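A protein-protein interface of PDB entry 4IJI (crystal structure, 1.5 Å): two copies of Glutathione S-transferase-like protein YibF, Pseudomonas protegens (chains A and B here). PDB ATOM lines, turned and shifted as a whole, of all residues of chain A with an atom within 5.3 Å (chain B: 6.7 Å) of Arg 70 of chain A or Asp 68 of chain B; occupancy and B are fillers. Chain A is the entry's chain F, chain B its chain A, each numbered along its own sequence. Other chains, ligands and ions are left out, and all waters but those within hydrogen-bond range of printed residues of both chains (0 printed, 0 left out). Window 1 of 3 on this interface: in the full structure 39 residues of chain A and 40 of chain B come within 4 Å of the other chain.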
ATOM      1  N   LYS A  16     -13.515 -13.789 -14.052  1.00  0.00           N
ATOM      2  CA  LYS A  16     -14.760 -13.810 -14.820  1.00  0.00           C
ATOM      3  C   LYS A  16     -15.725 -14.806 -14.194  1.00  0.00           C
ATOM      4  O   LYS A  16     -16.910 -14.518 -14.030  1.00  0.00           O
ATOM      5  CB  LYS A  16     -14.496 -14.237 -16.265  1.00  0.00           C
ATOM      6  CG  LYS A  16     -13.789 -13.201 -17.129  1.00  0.00           C
ATOM      7  CD  LYS A  16     -13.767 -13.630 -18.596  1.00  0.00           C
ATOM      8  CE  LYS A  16     -12.993 -14.928 -18.789  1.00  0.00           C
ATOM      9  NZ  LYS A  16     -13.112 -15.474 -20.194  1.00  0.00           N
ATOM     10  N   ASP A  68     -11.798 -24.350 -20.704  1.00  0.00           N
ATOM     11  CA  ASP A  68     -11.260 -23.210 -19.961  1.00  0.00           C
ATOM     12  C   ASP A  68     -12.358 -22.294 -19.412  1.00  0.00           C
ATOM     13  O   ASP A  68     -13.504 -22.723 -19.258  1.00  0.00           O
ATOM     14  CB  ASP A  68     -10.301 -22.407 -20.857  1.00  0.00           C
ATOM     15  CG  ASP A  68     -10.976 -21.830 -22.086  1.00  0.00           C
ATOM     16  OD1 ASP A  68     -12.218 -21.903 -22.217  1.00  0.00           O
ATOM     17  OD2 ASP A  68     -10.231 -21.257 -22.917  1.00  0.00           O
ATOM     18  N   SER A  69     -12.006 -21.053 -19.078  1.00  0.00           N
ATOM     19  CA  SER A  69     -12.975 -20.159 -18.448  1.00  0.00           C
ATOM     20  C   SER A  69     -14.251 -19.992 -19.262  1.00  0.00           C
ATOM     21  O   SER A  69     -15.332 -19.896 -18.695  1.00  0.00           O
ATOM     22  CB  SER A  69     -12.360 -18.793 -18.152  1.00  0.00           C
ATOM     23  OG  SER A  69     -12.073 -18.113 -19.365  1.00  0.00           O
ATOM     24  N   ARG A  70     -14.146 -19.960 -20.590  1.00  0.00           N
ATOM     25  CA  ARG A  70     -15.346 -19.772 -21.402  1.00  0.00           C
ATOM     26  C   ARG A  70     -16.306 -20.950 -21.315  1.00  0.00           C
ATOM     27  O   ARG A  70     -17.517 -20.766 -21.284  1.00  0.00           O
ATOM     28  CB  ARG A  70     -14.980 -19.482 -22.851  1.00  0.00           C
ATOM     29  CG  ARG A  70     -14.467 -18.088 -23.052  1.00  0.00           C
ATOM     30  CD  ARG A  70     -14.527 -17.740 -24.529  1.00  0.00           C
ATOM     31  NE  ARG A  70     -13.205 -17.426 -25.049  1.00  0.00           N
ATOM     32  CZ  ARG A  70     -12.932 -17.234 -26.336  1.00  0.00           C
ATOM     33  NH1 ARG A  70     -13.891 -17.347 -27.247  1.00  0.00           N
ATOM     34  NH2 ARG A  70     -11.693 -16.950 -26.714  1.00  0.00           N
ATOM     35  N   VAL A  71     -15.763 -22.162 -21.269  1.00  0.00           N
ATOM     36  CA  VAL A  71     -16.567 -23.365 -21.103  1.00  0.00           C
ATOM     37  C   VAL A  71     -17.235 -23.379 -19.734  1.00  0.00           C
ATOM     38  O   VAL A  71     -18.415 -23.708 -19.594  1.00  0.00           O
ATOM     39  CB  VAL A  71     -15.676 -24.618 -21.264  1.00  0.00           C
ATOM     40  CG1 VAL A  71     -16.472 -25.894 -21.022  1.00  0.00           C
ATOM     41  CG2 VAL A  71     -15.064 -24.639 -22.670  1.00  0.00           C
ATOM     42  N   ILE A  72     -16.470 -23.009 -18.714  1.00  0.00           N
ATOM     43  CA  ILE A  72     -16.981 -22.987 -17.355  1.00  0.00           C
ATOM     44  C   ILE A  72     -18.095 -21.959 -17.220  1.00  0.00           C
ATOM     45  O   ILE A  72     -19.124 -22.228 -16.599  1.00  0.00           O
ATOM     46  CB  ILE A  72     -15.850 -22.673 -16.359  1.00  0.00           C
ATOM     47  CG1 ILE A  72     -14.850 -23.831 -16.350  1.00  0.00           C
ATOM     48  CG2 ILE A  72     -16.423 -22.376 -14.960  1.00  0.00           C
ATOM     49  CD1 ILE A  72     -13.515 -23.469 -15.699  1.00  0.00           C
ATOM     50  N   LEU A  73     -17.899 -20.784 -17.814  1.00  0.00           N
ATOM     51  CA  LEU A  73     -18.939 -19.753 -17.787  1.00  0.00           C
ATOM     52  C   LEU A  73     -20.217 -20.226 -18.486  1.00  0.00           C
ATOM     53  O   LEU A  73     -21.320 -19.988 -18.002  1.00  0.00           O
ATOM     54  CB  LEU A  73     -18.429 -18.448 -18.418  1.00  0.00           C
ATOM     55  CG  LEU A  73     -17.354 -17.702 -17.623  1.00  0.00           C
ATOM     56  CD1 LEU A  73     -16.514 -16.768 -18.488  1.00  0.00           C
ATOM     57  CD2 LEU A  73     -17.999 -16.928 -16.476  1.00  0.00           C
ATOM     58  N   ASP A  74     -20.054 -20.909 -19.610  1.00  0.00           N
ATOM     59  CA  ASP A  74     -21.186 -21.446 -20.359  1.00  0.00           C
ATOM     60  C   ASP A  74     -21.971 -22.411 -19.480  1.00  0.00           C
ATOM     61  O   ASP A  74     -23.194 -22.321 -19.377  1.00  0.00           O
ATOM     62  CB  ASP A  74     -20.669 -22.140 -21.622  1.00  0.00           C
ATOM     63  CG  ASP A  74     -21.777 -22.564 -22.567  1.00  0.00           C
ATOM     64  OD1 ASP A  74     -22.347 -23.661 -22.370  1.00  0.00           O
ATOM     65  OD2 ASP A  74     -22.062 -21.811 -23.517  1.00  0.00           O
ATOM     66  N   TYR A  75     -21.252 -23.322 -18.832  1.00  0.00           N
ATOM     67  CA  TYR A  75     -21.861 -24.293 -17.939  1.00  0.00           C
ATOM     68  C   TYR A  75     -22.593 -23.621 -16.785  1.00  0.00           C
ATOM     69  O   TYR A  75     -23.764 -23.923 -16.522  1.00  0.00           O
ATOM     70  CB  TYR A  75     -20.787 -25.246 -17.401  1.00  0.00           C
ATOM     71  CG  TYR A  75     -21.306 -26.147 -16.313  1.00  0.00           C
ATOM     72  CD1 TYR A  75     -22.053 -27.278 -16.616  1.00  0.00           C
ATOM     73  CD2 TYR A  75     -21.066 -25.857 -14.984  1.00  0.00           C
ATOM     74  CE1 TYR A  75     -22.541 -28.099 -15.613  1.00  0.00           C
ATOM     75  CE2 TYR A  75     -21.550 -26.667 -13.979  1.00  0.00           C
ATOM     76  CZ  TYR A  75     -22.284 -27.778 -14.301  1.00  0.00           C
ATOM     77  OH  TYR A  75     -22.753 -28.565 -13.285  1.00  0.00           O
ATOM     78  N   ALA A 101     -15.061 -12.182 -26.327  1.00  0.00           N
ATOM     79  CA  ALA A 101     -13.795 -12.607 -26.943  1.00  0.00           C
ATOM     80  C   ALA A 101     -12.812 -11.456 -27.100  1.00  0.00           C
ATOM     81  O   ALA A 101     -11.588 -11.646 -26.964  1.00  0.00           O
ATOM     82  CB  ALA A 101     -14.045 -13.292 -28.293  1.00  0.00           C
ATOM     83  N   ASP A 104     -11.366 -11.112 -23.705  1.00  0.00           N
ATOM     84  CA  ASP A 104     -10.384 -12.191 -23.530  1.00  0.00           C
ATOM     85  C   ASP A 104      -9.087 -11.897 -24.273  1.00  0.00           C
ATOM     86  O   ASP A 104      -8.002 -12.180 -23.783  1.00  0.00           O
ATOM     87  CB  ASP A 104     -10.966 -13.536 -23.972  1.00  0.00           C
ATOM     88  CG  ASP A 104     -11.956 -14.094 -22.973  1.00  0.00           C
ATOM     89  OD1 ASP A 104     -11.645 -14.073 -21.771  1.00  0.00           O
ATOM     90  OD2 ASP A 104     -13.052 -14.534 -23.382  1.00  0.00           O
ATOM     91  N   TYR B  13      -6.408 -22.467 -36.242  1.00  0.00           N
ATOM     92  CA  TYR B  13      -7.707 -21.963 -35.800  1.00  0.00           C
ATOM     93  C   TYR B  13      -8.589 -21.703 -37.012  1.00  0.00           C
ATOM     94  O   TYR B  13      -9.782 -21.987 -36.990  1.00  0.00           O
ATOM     95  CB  TYR B  13      -7.540 -20.683 -34.989  1.00  0.00           C
ATOM     96  CG  TYR B  13      -6.533 -20.769 -33.876  1.00  0.00           C
ATOM     97  CD1 TYR B  13      -6.898 -21.225 -32.617  1.00  0.00           C
ATOM     98  CD2 TYR B  13      -5.215 -20.390 -34.090  1.00  0.00           C
ATOM     99  CE1 TYR B  13      -5.963 -21.285 -31.581  1.00  0.00           C
ATOM    100  CE2 TYR B  13      -4.275 -20.456 -33.065  1.00  0.00           C
ATOM    101  CZ  TYR B  13      -4.666 -20.903 -31.825  1.00  0.00           C
ATOM    102  OH  TYR B  13      -3.745 -20.965 -30.813  1.00  0.00           O
ATOM    103  N   VAL B  17     -12.323 -23.934 -38.557  1.00  0.00           N
ATOM    104  CA  VAL B  17     -13.463 -23.363 -39.264  1.00  0.00           C
ATOM    105  C   VAL B  17     -13.653 -23.996 -40.643  1.00  0.00           C
ATOM    106  O   VAL B  17     -14.781 -24.359 -41.012  1.00  0.00           O
ATOM    107  CB  VAL B  17     -13.326 -21.833 -39.374  1.00  0.00           C
ATOM    108  CG1 VAL B  17     -14.451 -21.258 -40.194  1.00  0.00           C
ATOM    109  CG2 VAL B  17     -13.304 -21.215 -37.988  1.00  0.00           C
ATOM    110  N   ASN B  50     -11.209  -7.083 -36.745  1.00  0.00           N
ATOM    111  CA  ASN B  50     -10.877  -7.668 -35.452  1.00  0.00           C
ATOM    112  C   ASN B  50      -9.735  -6.867 -34.861  1.00  0.00           C
ATOM    113  O   ASN B  50      -8.600  -7.015 -35.294  1.00  0.00           O
ATOM    114  CB  ASN B  50     -10.435  -9.135 -35.591  1.00  0.00           C
ATOM    115  CG  ASN B  50     -10.063  -9.752 -34.252  1.00  0.00           C
ATOM    116  OD1 ASN B  50     -10.191  -9.107 -33.216  1.00  0.00           O
ATOM    117  ND2 ASN B  50      -9.599 -11.008 -34.264  1.00  0.00           N
ATOM    118  N   LEU B  52      -8.039  -7.232 -32.349  1.00  0.00           N
ATOM    119  CA  LEU B  52      -6.976  -8.061 -31.789  1.00  0.00           C
ATOM    120  C   LEU B  52      -5.927  -8.467 -32.817  1.00  0.00           C
ATOM    121  O   LEU B  52      -4.867  -8.970 -32.452  1.00  0.00           O
ATOM    122  CB  LEU B  52      -7.562  -9.313 -31.144  1.00  0.00           C
ATOM    123  CG  LEU B  52      -8.598  -9.118 -30.056  1.00  0.00           C
ATOM    124  CD1 LEU B  52      -9.174 -10.474 -29.677  1.00  0.00           C
ATOM    125  CD2 LEU B  52      -7.956  -8.464 -28.834  1.00  0.00           C
ATOM    126  N   LYS B  54      -6.076 -10.914 -35.079  1.00  0.00           N
ATOM    127  CA  LYS B  54      -5.935 -12.359 -35.201  1.00  0.00           C
ATOM    128  C   LYS B  54      -6.950 -12.948 -36.171  1.00  0.00           C
ATOM    129  O   LYS B  54      -8.049 -12.427 -36.316  1.00  0.00           O
ATOM    130  CB  LYS B  54      -6.050 -13.059 -33.826  1.00  0.00           C
ATOM    131  CG  LYS B  54      -4.933 -12.698 -32.832  1.00  0.00           C
ATOM    132  CD  LYS B  54      -4.964 -13.597 -31.604  1.00  0.00           C
ATOM    133  CE  LYS B  54      -3.848 -13.242 -30.633  1.00  0.00           C
ATOM    134  NZ  LYS B  54      -3.764 -14.272 -29.554  1.00  0.00           N
ATOM    135  N   PRO B  56      -8.977 -16.728 -37.198  1.00  0.00           N
ATOM    136  CA  PRO B  56     -10.050 -16.258 -38.080  1.00  0.00           C
ATOM    137  C   PRO B  56     -10.878 -15.110 -37.518  1.00  0.00           C
ATOM    138  O   PRO B  56     -10.978 -14.909 -36.304  1.00  0.00           O
ATOM    139  CB  PRO B  56     -10.941 -17.498 -38.218  1.00  0.00           C
ATOM    140  CG  PRO B  56     -10.753 -18.217 -36.912  1.00  0.00           C
ATOM    141  CD  PRO B  56      -9.288 -18.031 -36.588  1.00  0.00           C
ATOM    142  N   ALA B  57     -11.476 -14.371 -38.441  1.00  0.00           N
ATOM    143  CA  ALA B  57     -12.540 -13.429 -38.146  1.00  0.00           C
ATOM    144  C   ALA B  57     -13.542 -13.606 -39.271  1.00  0.00           C
ATOM    145  O   ALA B  57     -13.164 -13.823 -40.424  1.00  0.00           O
ATOM    146  CB  ALA B  57     -12.003 -12.005 -38.096  1.00  0.00           C
ATOM    147  N   LEU B  66     -17.560 -11.459 -36.349  1.00  0.00           N
ATOM    148  CA  LEU B  66     -17.420 -12.420 -35.253  1.00  0.00           C
ATOM    149  C   LEU B  66     -15.972 -12.881 -35.101  1.00  0.00           C
ATOM    150  O   LEU B  66     -15.268 -13.073 -36.092  1.00  0.00           O
ATOM    151  CB  LEU B  66     -18.279 -13.659 -35.479  1.00  0.00           C
ATOM    152  CG  LEU B  66     -19.765 -13.447 -35.757  1.00  0.00           C
ATOM    153  CD1 LEU B  66     -20.493 -14.786 -35.793  1.00  0.00           C
ATOM    154  CD2 LEU B  66     -20.394 -12.514 -34.721  1.00  0.00           C
ATOM    155  N   TYR B  67     -15.551 -13.073 -33.851  1.00  0.00           N
ATOM    156  CA  TYR B  67     -14.255 -13.685 -33.517  1.00  0.00           C
ATOM    157  C   TYR B  67     -14.380 -14.057 -32.031  1.00  0.00           C
ATOM    158  O   TYR B  67     -15.312 -13.573 -31.387  1.00  0.00           O
ATOM    159  CB  TYR B  67     -13.084 -12.705 -33.799  1.00  0.00           C
ATOM    160  CG  TYR B  67     -13.240 -11.337 -33.167  1.00  0.00           C
ATOM    161  CD1 TYR B  67     -12.848 -11.108 -31.851  1.00  0.00           C
ATOM    162  CD2 TYR B  67     -13.790 -10.278 -33.884  1.00  0.00           C
ATOM    163  CE1 TYR B  67     -13.014  -9.865 -31.260  1.00  0.00           C
ATOM    164  CE2 TYR B  67     -13.957  -9.031 -33.305  1.00  0.00           C
ATOM    165  CZ  TYR B  67     -13.557  -8.830 -32.005  1.00  0.00           C
ATOM    166  OH  TYR B  67     -13.725  -7.595 -31.439  1.00  0.00           O
ATOM    167  N   ASP B  68     -13.526 -14.912 -31.470  1.00  0.00           N
ATOM    168  CA  ASP B  68     -12.472 -15.661 -32.157  1.00  0.00           C
ATOM    169  C   ASP B  68     -13.017 -16.968 -32.745  1.00  0.00           C
ATOM    170  O   ASP B  68     -14.225 -17.078 -33.004  1.00  0.00           O
ATOM    171  CB  ASP B  68     -11.320 -15.930 -31.176  1.00  0.00           C
ATOM    172  CG  ASP B  68     -11.719 -16.829 -30.024  1.00  0.00           C
ATOM    173  OD1 ASP B  68     -12.928 -17.094 -29.852  1.00  0.00           O
ATOM    174  OD2 ASP B  68     -10.814 -17.282 -29.282  1.00  0.00           O
ATOM    175  N   SER B  69     -12.144 -17.950 -32.974  1.00  0.00           N
ATOM    176  CA  SER B  69     -12.573 -19.157 -33.676  1.00  0.00           C
ATOM    177  C   SER B  69     -13.724 -19.880 -32.990  1.00  0.00           C
ATOM    178  O   SER B  69     -14.587 -20.416 -33.666  1.00  0.00           O
ATOM    179  CB  SER B  69     -11.403 -20.116 -33.919  1.00  0.00           C
ATOM    180  OG  SER B  69     -10.941 -20.683 -32.695  1.00  0.00           O
ATOM    181  N   ARG B  70     -13.747 -19.923 -31.661  1.00  0.00           N
ATOM    182  CA  ARG B  70     -14.831 -20.659 -31.006  1.00  0.00           C
ATOM    183  C   ARG B  70     -16.179 -20.017 -31.251  1.00  0.00           C
ATOM    184  O   ARG B  70     -17.185 -20.710 -31.397  1.00  0.00           O
ATOM    185  CB  ARG B  70     -14.600 -20.781 -29.504  1.00  0.00           C
ATOM    186  CG  ARG B  70     -13.333 -21.468 -29.130  1.00  0.00           C
ATOM    187  CD  ARG B  70     -13.347 -21.690 -27.620  1.00  0.00           C
ATOM    188  NE  ARG B  70     -12.016 -21.830 -27.050  1.00  0.00           N
ATOM    189  CZ  ARG B  70     -11.791 -21.841 -25.743  1.00  0.00           C
ATOM    190  NH1 ARG B  70     -12.825 -21.749 -24.909  1.00  0.00           N
ATOM    191  NH2 ARG B  70     -10.553 -21.989 -25.284  1.00  0.00           N
ATOM    192  N   VAL B  71     -16.203 -18.691 -31.307  1.00  0.00           N
ATOM    193  CA  VAL B  71     -17.441 -17.966 -31.544  1.00  0.00           C
ATOM    194  C   VAL B  71     -17.896 -18.214 -32.979  1.00  0.00           C
ATOM    195  O   VAL B  71     -19.076 -18.432 -33.250  1.00  0.00           O
ATOM    196  CB  VAL B  71     -17.248 -16.451 -31.290  1.00  0.00           C
ATOM    197  CG1 VAL B  71     -18.530 -15.666 -31.570  1.00  0.00           C
ATOM    198  CG2 VAL B  71     -16.769 -16.200 -29.856  1.00  0.00           C
ATOM    199  N   ILE B  72     -16.949 -18.184 -33.904  1.00  0.00           N
ATOM    200  CA  ILE B  72     -17.245 -18.448 -35.313  1.00  0.00           C
ATOM    201  C   ILE B  72     -17.772 -19.867 -35.528  1.00  0.00           C
ATOM    202  O   ILE B  72     -18.757 -20.064 -36.249  1.00  0.00           O
ATOM    203  CB  ILE B  72     -16.005 -18.170 -36.176  1.00  0.00           C
ATOM    204  CG1 ILE B  72     -15.664 -16.667 -36.115  1.00  0.00           C
ATOM    205  CG2 ILE B  72     -16.235 -18.630 -37.617  1.00  0.00           C
ATOM    206  CD1 ILE B  72     -14.252 -16.334 -36.636  1.00  0.00           C
ATOM    207  N   LEU B  73     -17.134 -20.854 -34.896  1.00  0.00           N
ATOM    208  CA  LEU B  73     -17.603 -22.252 -34.973  1.00  0.00           C
ATOM    209  C   LEU B  73     -19.024 -22.414 -34.439  1.00  0.00           C
ATOM    210  O   LEU B  73     -19.855 -23.099 -35.054  1.00  0.00           O
ATOM    211  CB  LEU B  73     -16.635 -23.179 -34.229  1.00  0.00           C
ATOM    212  CG  LEU B  73     -15.275 -23.278 -34.909  1.00  0.00           C
ATOM    213  CD1 LEU B  73     -14.213 -23.695 -33.910  1.00  0.00           C
ATOM    214  CD2 LEU B  73     -15.301 -24.240 -36.104  1.00  0.00           C
ATOM    215  N   TRP B  94     -20.506 -29.931 -22.507  1.00  0.00           N
ATOM    216  CA  TRP B  94     -19.358 -29.447 -21.754  1.00  0.00           C
ATOM    217  C   TRP B  94     -18.163 -30.393 -21.812  1.00  0.00           C
ATOM    218  O   TRP B  94     -17.019 -29.949 -21.802  1.00  0.00           O
ATOM    219  CB  TRP B  94     -19.777 -28.995 -20.346  1.00  0.00           C
ATOM    220  CG  TRP B  94     -20.821 -27.891 -20.484  1.00  0.00           C
ATOM    221  CD1 TRP B  94     -20.628 -26.641 -21.023  1.00  0.00           C
ATOM    222  CD2 TRP B  94     -22.197 -27.965 -20.129  1.00  0.00           C
ATOM    223  NE1 TRP B  94     -21.803 -25.936 -21.011  1.00  0.00           N
ATOM    224  CE2 TRP B  94     -22.784 -26.726 -20.465  1.00  0.00           C
ATOM    225  CE3 TRP B  94     -22.995 -28.958 -19.548  1.00  0.00           C
ATOM    226  CZ2 TRP B  94     -24.129 -26.458 -20.236  1.00  0.00           C
ATOM    227  CZ3 TRP B  94     -24.326 -28.692 -19.328  1.00  0.00           C
ATOM    228  CH2 TRP B  94     -24.884 -27.453 -19.670  1.00  0.00           C
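NH2 of Arg 70 of chain A is in salt-bridge range of OD2 of Asp 68 of chain B, at 2.7 Å.
The guanidinium group (NH2) of Arg 70 of chain B is in salt-bridge range of the side-chain carboxylate (OD2) of Asp 68 of chain A (2.5 Å).
The indole nitrogen of Trp 94 of chain B lies close to the backbone NH of Tyr 75 of chain A, at 3.4 Å.
NE1 of Trp 94 of chain B lies within hydrogen-bond range of OD1 of Asp 74 of chain A, at 2.7 Å.
The side-chain amide oxygen (OD1) of Asn 50 of chain B sits at hydrogen-bond distance from the backbone NH (N) of Leu 52 of chain B (3.0 Å).
N of Arg 70 of chain B lies close to OD1 of Asp 68 of chain B, at 3.5 Å.
NE of Arg 70 of chain A is in salt-bridge range of OD2 of Asp 104 of chain A (3.3 Å).
The side-chain carboxylate (OD1) of Asp 68 of chain A lies close to the backbone NH (N) of Arg 70 of chain A, 3.2 Å away.
Among the printed residues, merely in contact across the chains: Ala 101 of chain A with Tyr 67 of chain B (3.4 Å), Ala 101 of chain A with Asp 68 of chain B (3.6 Å), Arg 70 of chain A with Arg 70 of chain B (3.7 Å), Ala 101 of chain A with Leu 52 of chain B (3.8 Å) and Val 71 of chain A with Trp 94 of chain B (3.9 Å).
Of chain B, only Asp 68 (2.7 Å) and Arg 70 (3.7 Å) come within 4 Å of Arg 70 of chain A.
Asp 68 of chain B touches just these residues of chain A: Arg 70 (2.7 Å) and Ala 101 (3.6 Å).
Of the printed residues of chain A, Leu 52 of chain B touches Ala 101.
Printed residues of chain A within 4 Å of Arg 70 of chain B: Asp 68 and Arg 70.
Of the printed residues of chain B, Asp 74 of chain A touches Trp 94 (2.7 Å).
Printed residues of chain A within 4 Å of Tyr 67 of chain B: Ala 101 (3.4 Å).
Of the printed residues of chain B, Asp 68 of chain A touches Arg 70.
The nearest printed residue of chain A that does not touch Asp 68 of chain B is Asp 104 of chain A (6.5 Å).
Hydrophobic or aromatic side chains of chain B within 4 Å of the printed part of chain A: Leu 52 and Trp 94.
Among the printed residues, Asp or Glu carboxylates within 4 Å of a Lys or Arg side-chain nitrogen of the other chain: Asp 68 of chain A with Arg 70 of chain B (2.5 Å) and Arg 70 of chain A with Asp 68 of chain B (2.7 Å).
Asp 68 of chain A touches Arg 70 of chain B, and with the chains exchanged Arg 70 of chain A touches Asp 68 of chain B.
Arg 70 of chain B touches its own counterpart, Arg 70 of chain A.
Of the 9 pairs that touch across the chains among the printed residues, 3 have their exchanged pair printed and touching as well.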
